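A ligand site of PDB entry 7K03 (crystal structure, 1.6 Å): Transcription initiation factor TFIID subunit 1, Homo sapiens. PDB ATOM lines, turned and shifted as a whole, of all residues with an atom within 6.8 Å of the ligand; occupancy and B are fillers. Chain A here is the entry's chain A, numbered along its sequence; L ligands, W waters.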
ATOM      1  N   TRP A 156       8.872  19.397  -2.548  1.00  0.00           N
ATOM      2  CA  TRP A 156       8.034  20.432  -3.172  1.00  0.00           C
ATOM      3  C   TRP A 156       8.094  21.804  -2.503  1.00  0.00           C
ATOM      4  O   TRP A 156       7.983  22.815  -3.206  1.00  0.00           O
ATOM      5  CB  TRP A 156       6.576  19.967  -3.254  1.00  0.00           C
ATOM      6  CG  TRP A 156       5.905  19.802  -1.927  1.00  0.00           C
ATOM      7  CD1 TRP A 156       5.815  18.667  -1.192  1.00  0.00           C
ATOM      8  CD2 TRP A 156       5.276  20.827  -1.174  1.00  0.00           C
ATOM      9  NE1 TRP A 156       5.167  18.922  -0.013  1.00  0.00           N
ATOM     10  CE2 TRP A 156       4.830  20.249   0.020  1.00  0.00           C
ATOM     11  CE3 TRP A 156       5.036  22.187  -1.399  1.00  0.00           C
ATOM     12  CZ2 TRP A 156       4.163  20.984   0.992  1.00  0.00           C
ATOM     13  CZ3 TRP A 156       4.372  22.913  -0.425  1.00  0.00           C
ATOM     14  CH2 TRP A 156       3.954  22.317   0.751  1.00  0.00           C
ATOM     15  N   PRO A 157       8.271  21.934  -1.176  1.00  0.00           N
ATOM     16  CA  PRO A 157       8.287  23.302  -0.608  1.00  0.00           C
ATOM     17  C   PRO A 157       9.409  24.156  -1.156  1.00  0.00           C
ATOM     18  O   PRO A 157       9.348  25.386  -1.054  1.00  0.00           O
ATOM     19  CB  PRO A 157       8.445  23.052   0.899  1.00  0.00           C
ATOM     20  CG  PRO A 157       7.953  21.653   1.115  1.00  0.00           C
ATOM     21  CD  PRO A 157       8.402  20.915  -0.113  1.00  0.00           C
ATOM     22  N   PHE A 158      10.448  23.531  -1.690  1.00  0.00           N
ATOM     23  CA  PHE A 158      11.655  24.189  -2.179  1.00  0.00           C
ATOM     24  C   PHE A 158      11.707  24.295  -3.691  1.00  0.00           C
ATOM     25  O   PHE A 158      12.685  24.836  -4.218  1.00  0.00           O
ATOM     26  CB  PHE A 158      12.863  23.429  -1.649  1.00  0.00           C
ATOM     27  CG  PHE A 158      12.840  23.264  -0.151  1.00  0.00           C
ATOM     28  CD1 PHE A 158      13.004  24.352   0.684  1.00  0.00           C
ATOM     29  CD2 PHE A 158      12.588  22.032   0.409  1.00  0.00           C
ATOM     30  CE1 PHE A 158      12.926  24.216   2.050  1.00  0.00           C
ATOM     31  CE2 PHE A 158      12.525  21.863   1.797  1.00  0.00           C
ATOM     32  CZ  PHE A 158      12.707  22.984   2.616  1.00  0.00           C
ATOM     33  N   HIS A 159      10.662  23.845  -4.408  1.00  0.00           N
ATOM     34  CA  HIS A 159      10.720  23.839  -5.862  1.00  0.00           C
ATOM     35  C   HIS A 159      10.449  25.208  -6.474  1.00  0.00           C
ATOM     36  O   HIS A 159      10.842  25.428  -7.631  1.00  0.00           O
ATOM     37  CB  HIS A 159       9.681  22.884  -6.421  1.00  0.00           C
ATOM     38  CG  HIS A 159      10.042  21.442  -6.286  1.00  0.00           C
ATOM     39  ND1 HIS A 159       9.407  20.477  -7.021  1.00  0.00           N
ATOM     40  CD2 HIS A 159      10.938  20.789  -5.507  1.00  0.00           C
ATOM     41  CE1 HIS A 159       9.910  19.283  -6.723  1.00  0.00           C
ATOM     42  NE2 HIS A 159      10.839  19.458  -5.805  1.00  0.00           N
ATOM     43  N   HIS A 160       9.764  26.092  -5.760  1.00  0.00           N
ATOM     44  CA  HIS A 160       9.299  27.368  -6.305  1.00  0.00           C
ATOM     45  C   HIS A 160       9.371  28.436  -5.211  1.00  0.00           C
ATOM     46  O   HIS A 160       9.416  28.099  -4.036  1.00  0.00           O
ATOM     47  CB  HIS A 160       7.855  27.285  -6.783  1.00  0.00           C
ATOM     48  CG  HIS A 160       7.641  26.206  -7.791  1.00  0.00           C
ATOM     49  ND1 HIS A 160       8.040  26.329  -9.105  1.00  0.00           N
ATOM     50  CD2 HIS A 160       7.121  24.958  -7.668  1.00  0.00           C
ATOM     51  CE1 HIS A 160       7.763  25.209  -9.748  1.00  0.00           C
ATOM     52  NE2 HIS A 160       7.204  24.373  -8.893  1.00  0.00           N
ATOM     53  N   PRO A 161       9.331  29.707  -5.608  1.00  0.00           N
ATOM     54  CA  PRO A 161       9.254  30.750  -4.577  1.00  0.00           C
ATOM     55  C   PRO A 161       7.983  30.608  -3.759  1.00  0.00           C
ATOM     56  O   PRO A 161       6.925  30.279  -4.302  1.00  0.00           O
ATOM     57  CB  PRO A 161       9.221  32.052  -5.411  1.00  0.00           C
ATOM     58  CG  PRO A 161       9.725  31.694  -6.722  1.00  0.00           C
ATOM     59  CD  PRO A 161       9.368  30.260  -6.963  1.00  0.00           C
ATOM     60  N   VAL A 162       8.091  30.932  -2.472  1.00  0.00           N
ATOM     61  CA  VAL A 162       6.918  30.942  -1.617  1.00  0.00           C
ATOM     62  C   VAL A 162       5.967  32.022  -2.089  1.00  0.00           C
ATOM     63  O   VAL A 162       6.381  33.152  -2.412  1.00  0.00           O
ATOM     64  CB  VAL A 162       7.321  31.199  -0.153  1.00  0.00           C
ATOM     65  CG1 VAL A 162       6.087  31.399   0.723  1.00  0.00           C
ATOM     66  CG2 VAL A 162       8.134  30.040   0.379  1.00  0.00           C
ATOM     67  N   ASN A 163       4.684  31.705  -2.117  1.00  0.00           N
ATOM     68  CA  ASN A 163       3.659  32.689  -2.405  1.00  0.00           C
ATOM     69  C   ASN A 163       3.207  33.265  -1.086  1.00  0.00           C
ATOM     70  O   ASN A 163       2.622  32.554  -0.255  1.00  0.00           O
ATOM     71  CB  ASN A 163       2.488  32.067  -3.160  1.00  0.00           C
ATOM     72  CG  ASN A 163       1.546  33.117  -3.726  1.00  0.00           C
ATOM     73  OD1 ASN A 163       1.325  34.154  -3.104  1.00  0.00           O
ATOM     74  ND2 ASN A 163       0.962  32.836  -4.887  1.00  0.00           N
ATOM     75  N   LYS A 164       3.482  34.552  -0.874  1.00  0.00           N
ATOM     76  CA  LYS A 164       3.116  35.242   0.366  1.00  0.00           C
ATOM     77  C   LYS A 164       1.622  35.130   0.664  1.00  0.00           C
ATOM     78  O   LYS A 164       1.220  35.250   1.833  1.00  0.00           O
ATOM     79  CB  LYS A 164       3.554  36.705   0.263  1.00  0.00           C
ATOM     80  CG  LYS A 164       3.414  37.494   1.565  1.00  0.00           C
ATOM     81  CD  LYS A 164       4.350  38.716   1.600  1.00  0.00           C
ATOM     82  CE  LYS A 164       3.994  39.695   0.550  1.00  0.00           C
ATOM     83  NZ  LYS A 164       4.873  40.917   0.658  1.00  0.00           N
ATOM     84  N   LYS A 165       0.768  34.925  -0.337  1.00  0.00           N
ATOM     85  CA  LYS A 165      -0.651  34.775  -0.020  1.00  0.00           C
ATOM     86  C   LYS A 165      -0.893  33.550   0.836  1.00  0.00           C
ATOM     87  O   LYS A 165      -1.787  33.543   1.688  1.00  0.00           O
ATOM     88  CB  LYS A 165      -1.462  34.678  -1.300  1.00  0.00           C
ATOM     89  CG  LYS A 165      -2.951  34.642  -1.052  1.00  0.00           C
ATOM     90  CD  LYS A 165      -3.691  34.706  -2.366  1.00  0.00           C
ATOM     91  CE  LYS A 165      -5.182  34.787  -2.162  1.00  0.00           C
ATOM     92  NZ  LYS A 165      -5.896  34.689  -3.472  1.00  0.00           N
ATOM     93  N   PHE A 166      -0.110  32.500   0.624  1.00  0.00           N
ATOM     94  CA  PHE A 166      -0.289  31.223   1.315  1.00  0.00           C
ATOM     95  C   PHE A 166       0.547  31.090   2.583  1.00  0.00           C
ATOM     96  O   PHE A 166       0.202  30.273   3.443  1.00  0.00           O
ATOM     97  CB  PHE A 166      -0.003  30.037   0.380  1.00  0.00           C
ATOM     98  CG  PHE A 166      -0.809  30.057  -0.908  1.00  0.00           C
ATOM     99  CD1 PHE A 166      -2.122  30.489  -0.924  1.00  0.00           C
ATOM    100  CD2 PHE A 166      -0.234  29.641  -2.099  1.00  0.00           C
ATOM    101  CE1 PHE A 166      -2.856  30.487  -2.072  1.00  0.00           C
ATOM    102  CE2 PHE A 166      -0.962  29.646  -3.267  1.00  0.00           C
ATOM    103  CZ  PHE A 166      -2.261  30.068  -3.253  1.00  0.00           C
ATOM    104  N   VAL A 167       1.628  31.849   2.696  1.00  0.00           N
ATOM    105  CA  VAL A 167       2.492  31.842   3.877  1.00  0.00           C
ATOM    106  C   VAL A 167       2.761  33.303   4.206  1.00  0.00           C
ATOM    107  O   VAL A 167       3.815  33.857   3.828  1.00  0.00           O
ATOM    108  CB  VAL A 167       3.787  31.066   3.621  1.00  0.00           C
ATOM    109  CG1 VAL A 167       4.539  30.878   4.940  1.00  0.00           C
ATOM    110  CG2 VAL A 167       3.544  29.684   2.950  1.00  0.00           C
ATOM    111  N   TYR A 170       6.209  34.833   5.500  1.00  0.00           N
ATOM    112  CA  TYR A 170       7.442  34.172   5.079  1.00  0.00           C
ATOM    113  C   TYR A 170       8.558  35.180   4.840  1.00  0.00           C
ATOM    114  O   TYR A 170       9.703  34.971   5.247  1.00  0.00           O
ATOM    115  CB  TYR A 170       7.205  33.330   3.826  1.00  0.00           C
ATOM    116  CG  TYR A 170       8.437  32.561   3.447  1.00  0.00           C
ATOM    117  CD1 TYR A 170       8.783  31.403   4.147  1.00  0.00           C
ATOM    118  CD2 TYR A 170       9.279  33.008   2.442  1.00  0.00           C
ATOM    119  CE1 TYR A 170       9.929  30.720   3.830  1.00  0.00           C
ATOM    120  CE2 TYR A 170      10.417  32.321   2.121  1.00  0.00           C
ATOM    121  CZ  TYR A 170      10.741  31.189   2.819  1.00  0.00           C
ATOM    122  OH  TYR A 170      11.894  30.514   2.482  1.00  0.00           O
ATOM    123  N   ASP A 179      15.094  29.430  -4.113  1.00  0.00           N
ATOM    124  CA  ASP A 179      14.339  28.225  -4.395  1.00  0.00           C
ATOM    125  C   ASP A 179      14.884  27.617  -5.686  1.00  0.00           C
ATOM    126  O   ASP A 179      15.627  28.257  -6.420  1.00  0.00           O
ATOM    127  CB  ASP A 179      12.862  28.530  -4.529  1.00  0.00           C
ATOM    128  CG  ASP A 179      12.599  29.349  -5.742  1.00  0.00           C
ATOM    129  OD1 ASP A 179      12.743  30.577  -5.626  1.00  0.00           O
ATOM    130  OD2 ASP A 179      12.355  28.758  -6.817  1.00  0.00           O
ATOM    131  N   ASN A 208      17.772  29.230   4.694  1.00  0.00           N
ATOM    132  CA  ASN A 208      16.451  29.810   4.920  1.00  0.00           C
ATOM    133  C   ASN A 208      15.498  28.825   5.565  1.00  0.00           C
ATOM    134  O   ASN A 208      14.581  29.240   6.290  1.00  0.00           O
ATOM    135  CB  ASN A 208      15.889  30.319   3.603  1.00  0.00           C
ATOM    136  CG  ASN A 208      16.601  31.563   3.129  1.00  0.00           C
ATOM    137  OD1 ASN A 208      17.219  32.292   3.921  1.00  0.00           O
ATOM    138  ND2 ASN A 208      16.480  31.841   1.841  1.00  0.00           N
ATOM    139  N   SER A 209      15.661  27.524   5.307  1.00  0.00           N
ATOM    140  CA  SER A 209      14.837  26.534   6.007  1.00  0.00           C
ATOM    141  C   SER A 209      15.172  26.467   7.486  1.00  0.00           C
ATOM    142  O   SER A 209      14.268  26.394   8.338  1.00  0.00           O
ATOM    143  CB  SER A 209      15.035  25.157   5.368  1.00  0.00           C
ATOM    144  OG  SER A 209      14.110  24.243   5.920  1.00  0.00           O
ATOM    145  N   TYR A 212      13.499  29.655   8.945  1.00  0.00           N
ATOM    146  CA  TYR A 212      12.044  29.752   8.987  1.00  0.00           C
ATOM    147  C   TYR A 212      11.413  28.553   9.700  1.00  0.00           C
ATOM    148  O   TYR A 212      10.448  28.705  10.446  1.00  0.00           O
ATOM    149  CB  TYR A 212      11.443  29.885   7.569  1.00  0.00           C
ATOM    150  CG  TYR A 212       9.981  30.200   7.644  1.00  0.00           C
ATOM    151  CD1 TYR A 212       9.536  31.509   7.871  1.00  0.00           C
ATOM    152  CD2 TYR A 212       9.030  29.206   7.549  1.00  0.00           C
ATOM    153  CE1 TYR A 212       8.193  31.784   7.998  1.00  0.00           C
ATOM    154  CE2 TYR A 212       7.686  29.467   7.666  1.00  0.00           C
ATOM    155  CZ  TYR A 212       7.279  30.757   7.902  1.00  0.00           C
ATOM    156  OH  TYR A 212       5.920  31.008   8.035  1.00  0.00           O
ATOM    157  N   ASN A 213      11.937  27.359   9.459  1.00  0.00           N
ATOM    158  CA  ASN A 213      11.322  26.143   9.980  1.00  0.00           C
ATOM    159  C   ASN A 213      12.024  25.600  11.202  1.00  0.00           C
ATOM    160  O   ASN A 213      11.413  24.819  11.948  1.00  0.00           O
ATOM    161  CB  ASN A 213      11.308  25.054   8.906  1.00  0.00           C
ATOM    162  CG  ASN A 213      10.602  25.502   7.645  1.00  0.00           C
ATOM    163  OD1 ASN A 213       9.435  25.905   7.694  1.00  0.00           O
ATOM    164  ND2 ASN A 213      11.303  25.434   6.521  1.00  0.00           N
ATOM    165  N   SER A 217      13.424  20.646  12.002  1.00  0.00           N
ATOM    166  CA  SER A 217      12.173  20.456  11.282  1.00  0.00           C
ATOM    167  C   SER A 217      12.329  19.400  10.191  1.00  0.00           C
ATOM    168  O   SER A 217      13.395  19.259   9.596  1.00  0.00           O
ATOM    169  CB  SER A 217      11.727  21.787  10.675  1.00  0.00           C
ATOM    170  OG  SER A 217      10.727  21.657   9.672  1.00  0.00           O
ATOM    171  N   TYR A 219      11.058  19.813   7.330  1.00  0.00           N
ATOM    172  CA  TYR A 219      11.383  20.593   6.148  1.00  0.00           C
ATOM    173  C   TYR A 219      12.891  20.795   5.996  1.00  0.00           C
ATOM    174  O   TYR A 219      13.437  20.700   4.898  1.00  0.00           O
ATOM    175  CB  TYR A 219      10.671  21.952   6.179  1.00  0.00           C
ATOM    176  CG  TYR A 219       9.169  21.880   5.963  1.00  0.00           C
ATOM    177  CD1 TYR A 219       8.638  21.122   4.936  1.00  0.00           C
ATOM    178  CD2 TYR A 219       8.286  22.527   6.821  1.00  0.00           C
ATOM    179  CE1 TYR A 219       7.269  21.027   4.733  1.00  0.00           C
ATOM    180  CE2 TYR A 219       6.900  22.439   6.620  1.00  0.00           C
ATOM    181  CZ  TYR A 219       6.406  21.698   5.577  1.00  0.00           C
ATOM    182  OH  TYR A 219       5.032  21.604   5.383  1.00  0.00           O
HETATM  183  C1  LIG L   1       6.982  27.393   4.627  1.00  0.00           C
HETATM  184  C2  LIG L   1       7.296  26.070   3.896  1.00  0.00           C
HETATM  185  C3  LIG L   1       8.515  25.374   4.551  1.00  0.00           C
HETATM  186  C4  LIG L   1       9.964  26.041   2.824  1.00  0.00           C
HETATM  187  C5  LIG L   1       8.824  26.793   2.081  1.00  0.00           C
HETATM  188  C6  LIG L   1       6.449  26.320   1.613  1.00  0.00           C
HETATM  189  C7  LIG L   1       4.058  26.154   1.393  1.00  0.00           C
HETATM  190  C8  LIG L   1       5.366  26.650  -0.537  1.00  0.00           C
HETATM  191  C9  LIG L   1       6.534  26.595   0.239  1.00  0.00           C
HETATM  192  C10 LIG L   1       5.456  26.933  -1.977  1.00  0.00           C
HETATM  193  C11 LIG L   1       6.815  27.127  -2.676  1.00  0.00           C
HETATM  194  C12 LIG L   1       6.017  25.848  -2.906  1.00  0.00           C
HETATM  195  C13 LIG L   1       2.660  26.937  -2.721  1.00  0.00           C
HETATM  196  C14 LIG L   1       2.805  25.989   2.042  1.00  0.00           C
HETATM  197  C15 LIG L   1       2.635  25.254   3.232  1.00  0.00           C
HETATM  198  C16 LIG L   1       3.498  24.488   4.026  1.00  0.00           C
HETATM  199  C17 LIG L   1       2.749  23.984   5.083  1.00  0.00           C
HETATM  200  C18 LIG L   1       1.377  25.188   3.859  1.00  0.00           C
HETATM  201  C19 LIG L   1       0.422  26.540   2.204  1.00  0.00           C
HETATM  202  C20 LIG L   1       1.676  26.651   1.549  1.00  0.00           C
HETATM  203  N1  LIG L   1       7.541  26.227   2.456  1.00  0.00           N
HETATM  204  N2  LIG L   1       5.217  26.109   2.131  1.00  0.00           N
HETATM  205  N3  LIG L   1       4.150  26.465   0.076  1.00  0.00           N
HETATM  206  N4  LIG L   1       4.454  28.512  -4.068  1.00  0.00           N
HETATM  207  N5  LIG L   1       1.485  24.426   4.956  1.00  0.00           N
HETATM  208  N6  LIG L   1       0.297  25.839   3.346  1.00  0.00           N
HETATM  209  O1  LIG L   1       9.706  26.094   4.217  1.00  0.00           O
HETATM  210  O2  LIG L   1       3.811  29.144  -1.524  1.00  0.00           O
HETATM  211  S1  LIG L   1       4.106  28.015  -2.550  1.00  0.00           S
HETATM  212  O   HOH W   1      -2.230  26.374   4.640  1.00  0.00           O
HETATM  213  O   HOH W   2       4.052  26.972  -6.403  1.00  0.00           O
HETATM  214  O   HOH W   3       0.087  24.704   7.450  1.00  0.00           O
HETATM  215  O   HOH W   4       6.107  23.283  -5.209  1.00  0.00           O
HETATM  216  O   HOH W   5       1.809  29.032  -5.307  1.00  0.00           O
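O2 of the ligand is in hydrogen-bond range of N of Asn 163 (2.8 Å).
N4 of the ligand is in hydrogen-bond range of O of Pro 161 (3.0 Å).
ND2 of Asn 213 is in hydrogen-bond range of O1 of the ligand, at 2.9 Å.
The side-chain hydroxyl of Ser 209 sits at hydrogen-bond distance from the side-chain amide nitrogen of Asn 213, 3.1 Å away.
The side-chain amide oxygen of Asn 163 lies within hydrogen-bond range of the backbone NH of Lys 165, 2.9 Å away.
The backbone NH of Tyr 219 sits at hydrogen-bond distance from the side-chain hydroxyl of Ser 217, 3.0 Å away.
CZ3 of Trp 156 touches N3 of the ligand, 3.6 Å away.
Pro 157 touches the ligand.
Phe 158 touches the ligand.
His 160 touches the ligand.
CA of Val 162 touches O2 of the ligand (3.6 Å).
Phe 166 touches the ligand.
CG2 of Val 167 touches C20 of the ligand, at 3.8 Å.
CE2 of Tyr 212 touches C1 of the ligand (3.7 Å).
Tyr 219 touches the ligand (OH to C17, 3.3 Å).
Hydrophobic or aromatic side chains that line the ligand: Trp 156, Pro 157, Phe 158, Val 162, Phe 166, Val 167, Tyr 212 and Tyr 219.
12 residues have an atom within 4 Å of the ligand: Trp 156, Pro 157, Phe 158, His 160, Pro 161, Val 162, Asn 163, Phe 166, Val 167, Tyr 212, Asn 213 and Tyr 219.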
